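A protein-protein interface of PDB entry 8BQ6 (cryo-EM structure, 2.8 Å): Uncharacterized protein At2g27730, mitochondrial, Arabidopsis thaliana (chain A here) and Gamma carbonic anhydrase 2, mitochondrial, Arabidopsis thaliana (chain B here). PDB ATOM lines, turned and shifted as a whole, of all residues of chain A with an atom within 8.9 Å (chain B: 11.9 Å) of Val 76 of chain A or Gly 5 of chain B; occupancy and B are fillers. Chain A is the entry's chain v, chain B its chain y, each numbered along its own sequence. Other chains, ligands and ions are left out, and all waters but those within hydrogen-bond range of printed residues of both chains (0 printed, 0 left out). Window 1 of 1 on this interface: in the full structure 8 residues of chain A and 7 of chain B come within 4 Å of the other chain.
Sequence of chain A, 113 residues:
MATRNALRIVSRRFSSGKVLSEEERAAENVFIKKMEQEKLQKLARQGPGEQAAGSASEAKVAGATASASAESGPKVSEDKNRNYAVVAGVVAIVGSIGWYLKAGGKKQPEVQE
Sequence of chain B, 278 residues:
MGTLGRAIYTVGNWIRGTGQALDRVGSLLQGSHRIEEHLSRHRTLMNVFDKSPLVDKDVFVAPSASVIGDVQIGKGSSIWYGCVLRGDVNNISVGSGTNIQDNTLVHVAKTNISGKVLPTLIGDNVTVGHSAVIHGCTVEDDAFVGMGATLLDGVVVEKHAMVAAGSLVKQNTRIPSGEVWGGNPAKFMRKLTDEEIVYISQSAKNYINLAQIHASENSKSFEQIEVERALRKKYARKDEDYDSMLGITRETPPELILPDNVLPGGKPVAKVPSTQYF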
ATOM      1  N   LYS A  75      16.079   3.341 -11.149  1.00  0.00           N
ATOM      2  CA  LYS A  75      16.526   4.706 -10.902  1.00  0.00           C
ATOM      3  C   LYS A  75      17.504   5.216 -11.962  1.00  0.00           C
ATOM      4  O   LYS A  75      17.515   6.407 -12.273  1.00  0.00           O
ATOM      5  CB  LYS A  75      17.187   4.807  -9.531  1.00  0.00           C
ATOM      6  CG  LYS A  75      18.451   3.986  -9.406  1.00  0.00           C
ATOM      7  CD  LYS A  75      19.072   4.148  -8.031  1.00  0.00           C
ATOM      8  CE  LYS A  75      20.345   3.327  -7.893  1.00  0.00           C
ATOM      9  NZ  LYS A  75      20.960   3.478  -6.548  1.00  0.00           N
ATOM     10  N   VAL A  76      18.333   4.321 -12.498  1.00  0.00           N
ATOM     11  CA  VAL A  76      19.384   4.682 -13.445  1.00  0.00           C
ATOM     12  C   VAL A  76      19.484   3.595 -14.508  1.00  0.00           C
ATOM     13  O   VAL A  76      19.381   2.402 -14.205  1.00  0.00           O
ATOM     14  CB  VAL A  76      20.742   4.883 -12.735  1.00  0.00           C
ATOM     15  CG1 VAL A  76      21.147   3.627 -11.975  1.00  0.00           C
ATOM     16  CG2 VAL A  76      21.825   5.285 -13.727  1.00  0.00           C
ATOM     17  N   SER A  77      19.678   4.008 -15.758  1.00  0.00           N
ATOM     18  CA  SER A  77      19.945   3.061 -16.832  1.00  0.00           C
ATOM     19  C   SER A  77      21.440   2.746 -16.858  1.00  0.00           C
ATOM     20  O   SER A  77      22.271   3.656 -16.956  1.00  0.00           O
ATOM     21  CB  SER A  77      19.470   3.625 -18.170  1.00  0.00           C
ATOM     22  OG  SER A  77      18.071   3.859 -18.162  1.00  0.00           O
ATOM     23  N   GLU A  78      21.817   1.478 -16.719  1.00  0.00           N
ATOM     24  CA  GLU A  78      23.259   1.131 -16.551  1.00  0.00           C
ATOM     25  C   GLU A  78      24.022   0.973 -17.868  1.00  0.00           C
ATOM     26  O   GLU A  78      25.173   1.445 -17.907  1.00  0.00           O
ATOM     27  CB  GLU A  78      23.359  -0.167 -15.736  1.00  0.00           C
ATOM     28  CG  GLU A  78      24.779  -0.619 -15.421  1.00  0.00           C
ATOM     29  CD  GLU A  78      25.415  -1.590 -16.403  1.00  0.00           C
ATOM     30  OE1 GLU A  78      24.807  -2.644 -16.674  1.00  0.00           O
ATOM     31  OE2 GLU A  78      26.514  -1.282 -16.902  1.00  0.00           O
ATOM     32  N   ASP A  79      23.432   0.365 -18.901  1.00  0.00           N
ATOM     33  CA  ASP A  79      24.179   0.043 -20.116  1.00  0.00           C
ATOM     34  C   ASP A  79      24.697   1.331 -20.745  1.00  0.00           C
ATOM     35  O   ASP A  79      23.929   2.106 -21.319  1.00  0.00           O
ATOM     36  CB  ASP A  79      23.276  -0.729 -21.071  1.00  0.00           C
ATOM     37  CG  ASP A  79      24.035  -1.443 -22.167  1.00  0.00           C
ATOM     38  OD1 ASP A  79      25.218  -1.128 -22.400  1.00  0.00           O
ATOM     39  OD2 ASP A  79      23.436  -2.336 -22.796  1.00  0.00           O
ATOM     40  N   LYS A  80      26.012   1.559 -20.642  1.00  0.00           N
ATOM     41  CA  LYS A  80      26.597   2.799 -21.152  1.00  0.00           C
ATOM     42  C   LYS A  80      26.498   2.885 -22.668  1.00  0.00           C
ATOM     43  O   LYS A  80      26.153   3.939 -23.208  1.00  0.00           O
ATOM     44  CB  LYS A  80      28.063   2.928 -20.724  1.00  0.00           C
ATOM     45  CG  LYS A  80      28.302   3.231 -19.262  1.00  0.00           C
ATOM     46  CD  LYS A  80      27.217   4.108 -18.721  1.00  0.00           C
ATOM     47  CE  LYS A  80      27.495   5.582 -18.862  1.00  0.00           C
ATOM     48  NZ  LYS A  80      26.244   6.397 -18.934  1.00  0.00           N
ATOM     49  N   ARG A  82      24.356   1.561 -24.619  1.00  0.00           N
ATOM     50  CA  ARG A  82      22.972   1.899 -24.924  1.00  0.00           C
ATOM     51  C   ARG A  82      22.708   3.385 -24.711  1.00  0.00           C
ATOM     52  O   ARG A  82      22.037   4.024 -25.528  1.00  0.00           O
ATOM     53  CB  ARG A  82      22.028   1.052 -24.075  1.00  0.00           C
ATOM     54  CG  ARG A  82      20.582   1.127 -24.522  1.00  0.00           C
ATOM     55  CD  ARG A  82      19.697   0.222 -23.695  1.00  0.00           C
ATOM     56  NE  ARG A  82      19.664   0.626 -22.296  1.00  0.00           N
ATOM     57  CZ  ARG A  82      19.851  -0.199 -21.275  1.00  0.00           C
ATOM     58  NH1 ARG A  82      20.108  -1.482 -21.462  1.00  0.00           N
ATOM     59  NH2 ARG A  82      19.777   0.277 -20.037  1.00  0.00           N
ATOM     60  N   ASN A  83      23.234   3.959 -23.624  1.00  0.00           N
ATOM     61  CA  ASN A  83      23.017   5.382 -23.369  1.00  0.00           C
ATOM     62  C   ASN A  83      23.670   6.253 -24.435  1.00  0.00           C
ATOM     63  O   ASN A  83      23.080   7.244 -24.883  1.00  0.00           O
ATOM     64  CB  ASN A  83      23.528   5.760 -21.980  1.00  0.00           C
ATOM     65  CG  ASN A  83      22.881   4.947 -20.891  1.00  0.00           C
ATOM     66  OD1 ASN A  83      21.742   4.507 -21.034  1.00  0.00           O
ATOM     67  ND2 ASN A  83      23.572   4.792 -19.772  1.00  0.00           N
ATOM     68  N   TYR A  84      24.887   5.905 -24.851  1.00  0.00           N
ATOM     69  CA  TYR A  84      25.552   6.658 -25.908  1.00  0.00           C
ATOM     70  C   TYR A  84      24.787   6.548 -27.217  1.00  0.00           C
ATOM     71  O   TYR A  84      24.682   7.522 -27.970  1.00  0.00           O
ATOM     72  CB  TYR A  84      26.985   6.166 -26.089  1.00  0.00           C
ATOM     73  CG  TYR A  84      27.828   6.281 -24.849  1.00  0.00           C
ATOM     74  CD1 TYR A  84      27.543   7.227 -23.879  1.00  0.00           C
ATOM     75  CD2 TYR A  84      28.905   5.435 -24.643  1.00  0.00           C
ATOM     76  CE1 TYR A  84      28.308   7.331 -22.743  1.00  0.00           C
ATOM     77  CE2 TYR A  84      29.677   5.533 -23.512  1.00  0.00           C
ATOM     78  CZ  TYR A  84      29.374   6.483 -22.564  1.00  0.00           C
ATOM     79  OH  TYR A  84      30.141   6.584 -21.430  1.00  0.00           O
ATOM     80  N   VAL A  87      21.883   8.872 -26.988  1.00  0.00           N
ATOM     81  CA  VAL A  87      22.331  10.245 -27.203  1.00  0.00           C
ATOM     82  C   VAL A  87      22.557  10.502 -28.684  1.00  0.00           C
ATOM     83  O   VAL A  87      22.202  11.563 -29.204  1.00  0.00           O
ATOM     84  CB  VAL A  87      23.601  10.531 -26.382  1.00  0.00           C
ATOM     85  CG1 VAL A  87      24.160  11.898 -26.730  1.00  0.00           C
ATOM     86  CG2 VAL A  87      23.311  10.435 -24.905  1.00  0.00           C
ATOM     87  N   MET B   1      25.516   4.425 -16.385  1.00  0.00           N
ATOM     88  CA  MET B   1      25.326   4.828 -15.013  1.00  0.00           C
ATOM     89  C   MET B   1      25.484   6.326 -15.074  1.00  0.00           C
ATOM     90  O   MET B   1      25.823   6.861 -16.126  1.00  0.00           O
ATOM     91  CB  MET B   1      26.365   4.210 -14.095  1.00  0.00           C
ATOM     92  CG  MET B   1      26.297   2.703 -13.947  1.00  0.00           C
ATOM     93  SD  MET B   1      24.678   2.356 -13.283  1.00  0.00           S
ATOM     94  CE  MET B   1      24.664   2.991 -11.737  1.00  0.00           C
ATOM     95  N   GLY B   2      25.247   7.004 -13.969  1.00  0.00           N
ATOM     96  CA  GLY B   2      25.608   8.396 -13.891  1.00  0.00           C
ATOM     97  C   GLY B   2      24.450   9.335 -14.146  1.00  0.00           C
ATOM     98  O   GLY B   2      23.271   8.982 -14.068  1.00  0.00           O
ATOM     99  N   THR B   3      24.818  10.578 -14.444  1.00  0.00           N
ATOM    100  CA  THR B   3      23.815  11.598 -14.716  1.00  0.00           C
ATOM    101  C   THR B   3      23.053  11.290 -15.998  1.00  0.00           C
ATOM    102  O   THR B   3      21.823  11.402 -16.040  1.00  0.00           O
ATOM    103  CB  THR B   3      24.492  12.963 -14.789  1.00  0.00           C
ATOM    104  OG1 THR B   3      24.959  13.316 -13.483  1.00  0.00           O
ATOM    105  CG2 THR B   3      23.522  14.019 -15.271  1.00  0.00           C
ATOM    106  N   LEU B   4      23.768  10.889 -17.052  1.00  0.00           N
ATOM    107  CA  LEU B   4      23.105  10.502 -18.292  1.00  0.00           C
ATOM    108  C   LEU B   4      22.195   9.302 -18.067  1.00  0.00           C
ATOM    109  O   LEU B   4      21.088   9.236 -18.621  1.00  0.00           O
ATOM    110  CB  LEU B   4      24.152  10.204 -19.364  1.00  0.00           C
ATOM    111  CG  LEU B   4      23.647   9.816 -20.753  1.00  0.00           C
ATOM    112  CD1 LEU B   4      22.759  10.912 -21.321  1.00  0.00           C
ATOM    113  CD2 LEU B   4      24.819   9.535 -21.672  1.00  0.00           C
ATOM    114  N   GLY B   5      22.639   8.353 -17.238  1.00  0.00           N
ATOM    115  CA  GLY B   5      21.786   7.231 -16.882  1.00  0.00           C
ATOM    116  C   GLY B   5      20.488   7.671 -16.235  1.00  0.00           C
ATOM    117  O   GLY B   5      19.404   7.206 -16.600  1.00  0.00           O
ATOM    118  N   ARG B   6      20.580   8.598 -15.279  1.00  0.00           N
ATOM    119  CA  ARG B   6      19.390   9.079 -14.585  1.00  0.00           C
ATOM    120  C   ARG B   6      18.470   9.859 -15.514  1.00  0.00           C
ATOM    121  O   ARG B   6      17.243   9.715 -15.448  1.00  0.00           O
ATOM    122  CB  ARG B   6      19.800   9.940 -13.395  1.00  0.00           C
ATOM    123  CG  ARG B   6      20.280   9.138 -12.208  1.00  0.00           C
ATOM    124  CD  ARG B   6      20.560  10.043 -11.025  1.00  0.00           C
ATOM    125  NE  ARG B   6      21.880  10.655 -11.110  1.00  0.00           N
ATOM    126  CZ  ARG B   6      22.985  10.109 -10.623  1.00  0.00           C
ATOM    127  NH1 ARG B   6      22.964   8.941 -10.001  1.00  0.00           N
ATOM    128  NH2 ARG B   6      24.142  10.749 -10.766  1.00  0.00           N
ATOM    129  N   ALA B   7      19.039  10.708 -16.370  1.00  0.00           N
ATOM    130  CA  ALA B   7      18.216  11.478 -17.294  1.00  0.00           C
ATOM    131  C   ALA B   7      17.468  10.564 -18.256  1.00  0.00           C
ATOM    132  O   ALA B   7      16.276  10.769 -18.522  1.00  0.00           O
ATOM    133  CB  ALA B   7      19.081  12.477 -18.061  1.00  0.00           C
ATOM    134  N   ILE B   8      18.145   9.536 -18.774  1.00  0.00           N
ATOM    135  CA  ILE B   8      17.476   8.621 -19.690  1.00  0.00           C
ATOM    136  C   ILE B   8      16.418   7.805 -18.960  1.00  0.00           C
ATOM    137  O   ILE B   8      15.344   7.533 -19.505  1.00  0.00           O
ATOM    138  CB  ILE B   8      18.506   7.728 -20.398  1.00  0.00           C
ATOM    139  CG1 ILE B   8      19.315   8.568 -21.381  1.00  0.00           C
ATOM    140  CG2 ILE B   8      17.820   6.569 -21.109  1.00  0.00           C
ATOM    141  CD1 ILE B   8      20.483   7.851 -21.970  1.00  0.00           C
ATOM    142  N   TYR B   9      16.693   7.411 -17.714  1.00  0.00           N
ATOM    143  CA  TYR B   9      15.683   6.709 -16.929  1.00  0.00           C
ATOM    144  C   TYR B   9      14.438   7.569 -16.726  1.00  0.00           C
ATOM    145  O   TYR B   9      13.305   7.091 -16.877  1.00  0.00           O
ATOM    146  CB  TYR B   9      16.276   6.301 -15.583  1.00  0.00           C
ATOM    147  CG  TYR B   9      15.535   5.183 -14.906  1.00  0.00           C
ATOM    148  CD1 TYR B   9      15.887   3.860 -15.124  1.00  0.00           C
ATOM    149  CD2 TYR B   9      14.467   5.448 -14.062  1.00  0.00           C
ATOM    150  CE1 TYR B   9      15.211   2.837 -14.506  1.00  0.00           C
ATOM    151  CE2 TYR B   9      13.782   4.428 -13.443  1.00  0.00           C
ATOM    152  CZ  TYR B   9      14.158   3.126 -13.671  1.00  0.00           C
ATOM    153  OH  TYR B   9      13.479   2.103 -13.057  1.00  0.00           O
ATOM    154  N   THR B  10      14.628   8.845 -16.386  1.00  0.00           N
ATOM    155  CA  THR B  10      13.488   9.738 -16.181  1.00  0.00           C
ATOM    156  C   THR B  10      12.693   9.929 -17.470  1.00  0.00           C
ATOM    157  O   THR B  10      11.450   9.909 -17.461  1.00  0.00           O
ATOM    158  CB  THR B  10      13.977  11.081 -15.638  1.00  0.00           C
ATOM    159  OG1 THR B  10      14.379  10.923 -14.272  1.00  0.00           O
ATOM    160  CG2 THR B  10      12.886  12.134 -15.724  1.00  0.00           C
ATOM    161  N   VAL B  11      13.391  10.108 -18.592  1.00  0.00           N
ATOM    162  CA  VAL B  11      12.705  10.263 -19.871  1.00  0.00           C
ATOM    163  C   VAL B  11      11.951   8.987 -20.229  1.00  0.00           C
ATOM    164  O   VAL B  11      10.853   9.031 -20.804  1.00  0.00           O
ATOM    165  CB  VAL B  11      13.713  10.664 -20.963  1.00  0.00           C
ATOM    166  CG1 VAL B  11      13.071  10.612 -22.335  1.00  0.00           C
ATOM    167  CG2 VAL B  11      14.262  12.051 -20.682  1.00  0.00           C
ATOM    168  N   GLY B  12      12.521   7.829 -19.893  1.00  0.00           N
ATOM    169  CA  GLY B  12      11.804   6.582 -20.083  1.00  0.00           C
ATOM    170  C   GLY B  12      10.540   6.515 -19.250  1.00  0.00           C
ATOM    171  O   GLY B  12       9.526   5.974 -19.688  1.00  0.00           O
ATOM    172  N   ASN B  13      10.589   7.061 -18.034  1.00  0.00           N
ATOM    173  CA  ASN B  13       9.386   7.142 -17.210  1.00  0.00           C
ATOM    174  C   ASN B  13       8.308   7.972 -17.895  1.00  0.00           C
ATOM    175  O   ASN B  13       7.130   7.587 -17.928  1.00  0.00           O
ATOM    176  CB  ASN B  13       9.723   7.741 -15.850  1.00  0.00           C
ATOM    177  CG  ASN B  13       9.931   6.694 -14.796  1.00  0.00           C
ATOM    178  OD1 ASN B  13       9.699   5.510 -15.028  1.00  0.00           O
ATOM    179  ND2 ASN B  13      10.385   7.118 -13.629  1.00  0.00           N
ATOM    180  N   TRP B  14       8.696   9.123 -18.440  1.00  0.00           N
ATOM    181  CA  TRP B  14       7.718   9.957 -19.137  1.00  0.00           C
ATOM    182  C   TRP B  14       7.121   9.220 -20.332  1.00  0.00           C
ATOM    183  O   TRP B  14       5.903   9.264 -20.558  1.00  0.00           O
ATOM    184  CB  TRP B  14       8.362  11.262 -19.591  1.00  0.00           C
ATOM    185  CG  TRP B  14       8.702  12.176 -18.477  1.00  0.00           C
ATOM    186  CD1 TRP B  14       8.157  12.190 -17.230  1.00  0.00           C
ATOM    187  CD2 TRP B  14       9.696  13.203 -18.494  1.00  0.00           C
ATOM    188  NE1 TRP B  14       8.741  13.172 -16.470  1.00  0.00           N
ATOM    189  CE2 TRP B  14       9.691  13.809 -17.225  1.00  0.00           C
ATOM    190  CE3 TRP B  14      10.583  13.677 -19.464  1.00  0.00           C
ATOM    191  CZ2 TRP B  14      10.542  14.860 -16.898  1.00  0.00           C
ATOM    192  CZ3 TRP B  14      11.428  14.719 -19.138  1.00  0.00           C
ATOM    193  CH2 TRP B  14      11.402  15.299 -17.867  1.00  0.00           C
ATOM    194  N   ILE B  15       7.966   8.533 -21.104  1.00  0.00           N
ATOM    195  CA  ILE B  15       7.481   7.807 -22.276  1.00  0.00           C
ATOM    196  C   ILE B  15       6.538   6.684 -21.862  1.00  0.00           C
ATOM    197  O   ILE B  15       5.522   6.435 -22.520  1.00  0.00           O
ATOM    198  CB  ILE B  15       8.664   7.281 -23.110  1.00  0.00           C
ATOM    199  CG1 ILE B  15       9.383   8.432 -23.808  1.00  0.00           C
ATOM    200  CG2 ILE B  15       8.193   6.275 -24.138  1.00  0.00           C
ATOM    201  CD1 ILE B  15      10.750   8.064 -24.306  1.00  0.00           C
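The backbone NH (N) of Lys 75 of chain A sits close to the side-chain hydroxyl (OH) of Tyr 9 of chain B (3.5 Å).
The backbone carbonyl oxygen (O) of Gly 5 of chain B is in hydrogen-bond range of the backbone NH (N) of Ser 77 of chain A (3.3 Å).
NZ of Lys 80 of chain A is in hydrogen-bond range of O of Met 1 of chain B, 2.9 Å away.
The backbone carbonyl oxygen (O) of Ser 77 of chain A sits at hydrogen-bond distance from the backbone NH (N) of Met 1 of chain B.
O of Glu 78 of chain A sits at hydrogen-bond distance from N of Met 1 of chain B (3.4 Å).
Among the printed residues, pairs that only touch across the chains: Val 76 of chain A with Met 1 of chain B (3.6 Å), Val 76 of chain A with Tyr 9 of chain B (3.6 Å), Val 87 of chain A with Leu 4 of chain B (3.7 Å), Asn 83 of chain A with Ile 8 of chain B (3.7 Å), Val 76 of chain A with Gly 5 of chain B (3.7 Å), Ser 77 of chain A with Tyr 9 of chain B (3.7 Å), Val 76 of chain A with Gly 2 of chain B (3.8 Å), Val 76 of chain A with Arg 6 of chain B (3.9 Å), Lys 75 of chain A with Arg 6 of chain B (3.9 Å) and Asn 83 of chain A with Met 1 of chain B (3.9 Å).
Lys 75 of chain A touches just these residues of chain B: Arg 6 (3.9 Å) and Tyr 9 (3.2 Å).
Printed residues of chain B within 4 Å of Lys 80 of chain A: Met 1.
Of chain A, only Val 76 comes within 4 Å of Gly 2 of chain B.
Of the printed residues of chain A, Leu 4 of chain B touches Val 87.
Of chain A, only Val 76 and Ser 77 come within 4 Å of Gly 5 of chain B.
Printed residues of chain A within 4 Å of Ile 8 of chain B: Asn 83 (3.7 Å).
Printed residues of chain A within 4 Å of Tyr 9 of chain B: Lys 75, Val 76 and Ser 77.
The side-chain amide nitrogen (ND2) of Asn 83 of chain A lies close to the backbone carbonyl oxygen (O) of Asp 79 of chain A (3.1 Å).
OG1 of Thr 10 of chain B sits at hydrogen-bond distance from O of Arg 6 of chain B, at 3.3 Å.
ND2 of Asn 83 of chain A sits close to NZ of Lys 80 of chain A, at 3.2 Å.
The side-chain amide nitrogen of Asn 83 of chain A sits at hydrogen-bond distance from the backbone carbonyl oxygen of Ser 77 of chain A (3.3 Å).
Hydrophobic or aromatic side chains of chain A within 4 Å of the printed part of chain B: Val 76 and Val 87.
Along chain A the printed residues that touch a printed residue of chain B span positions 75 to 87.
Hydrophobic or aromatic side chains of chain B within 4 Å of the printed part of chain A: Met 1, Leu 4, Ile 8 and Tyr 9.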
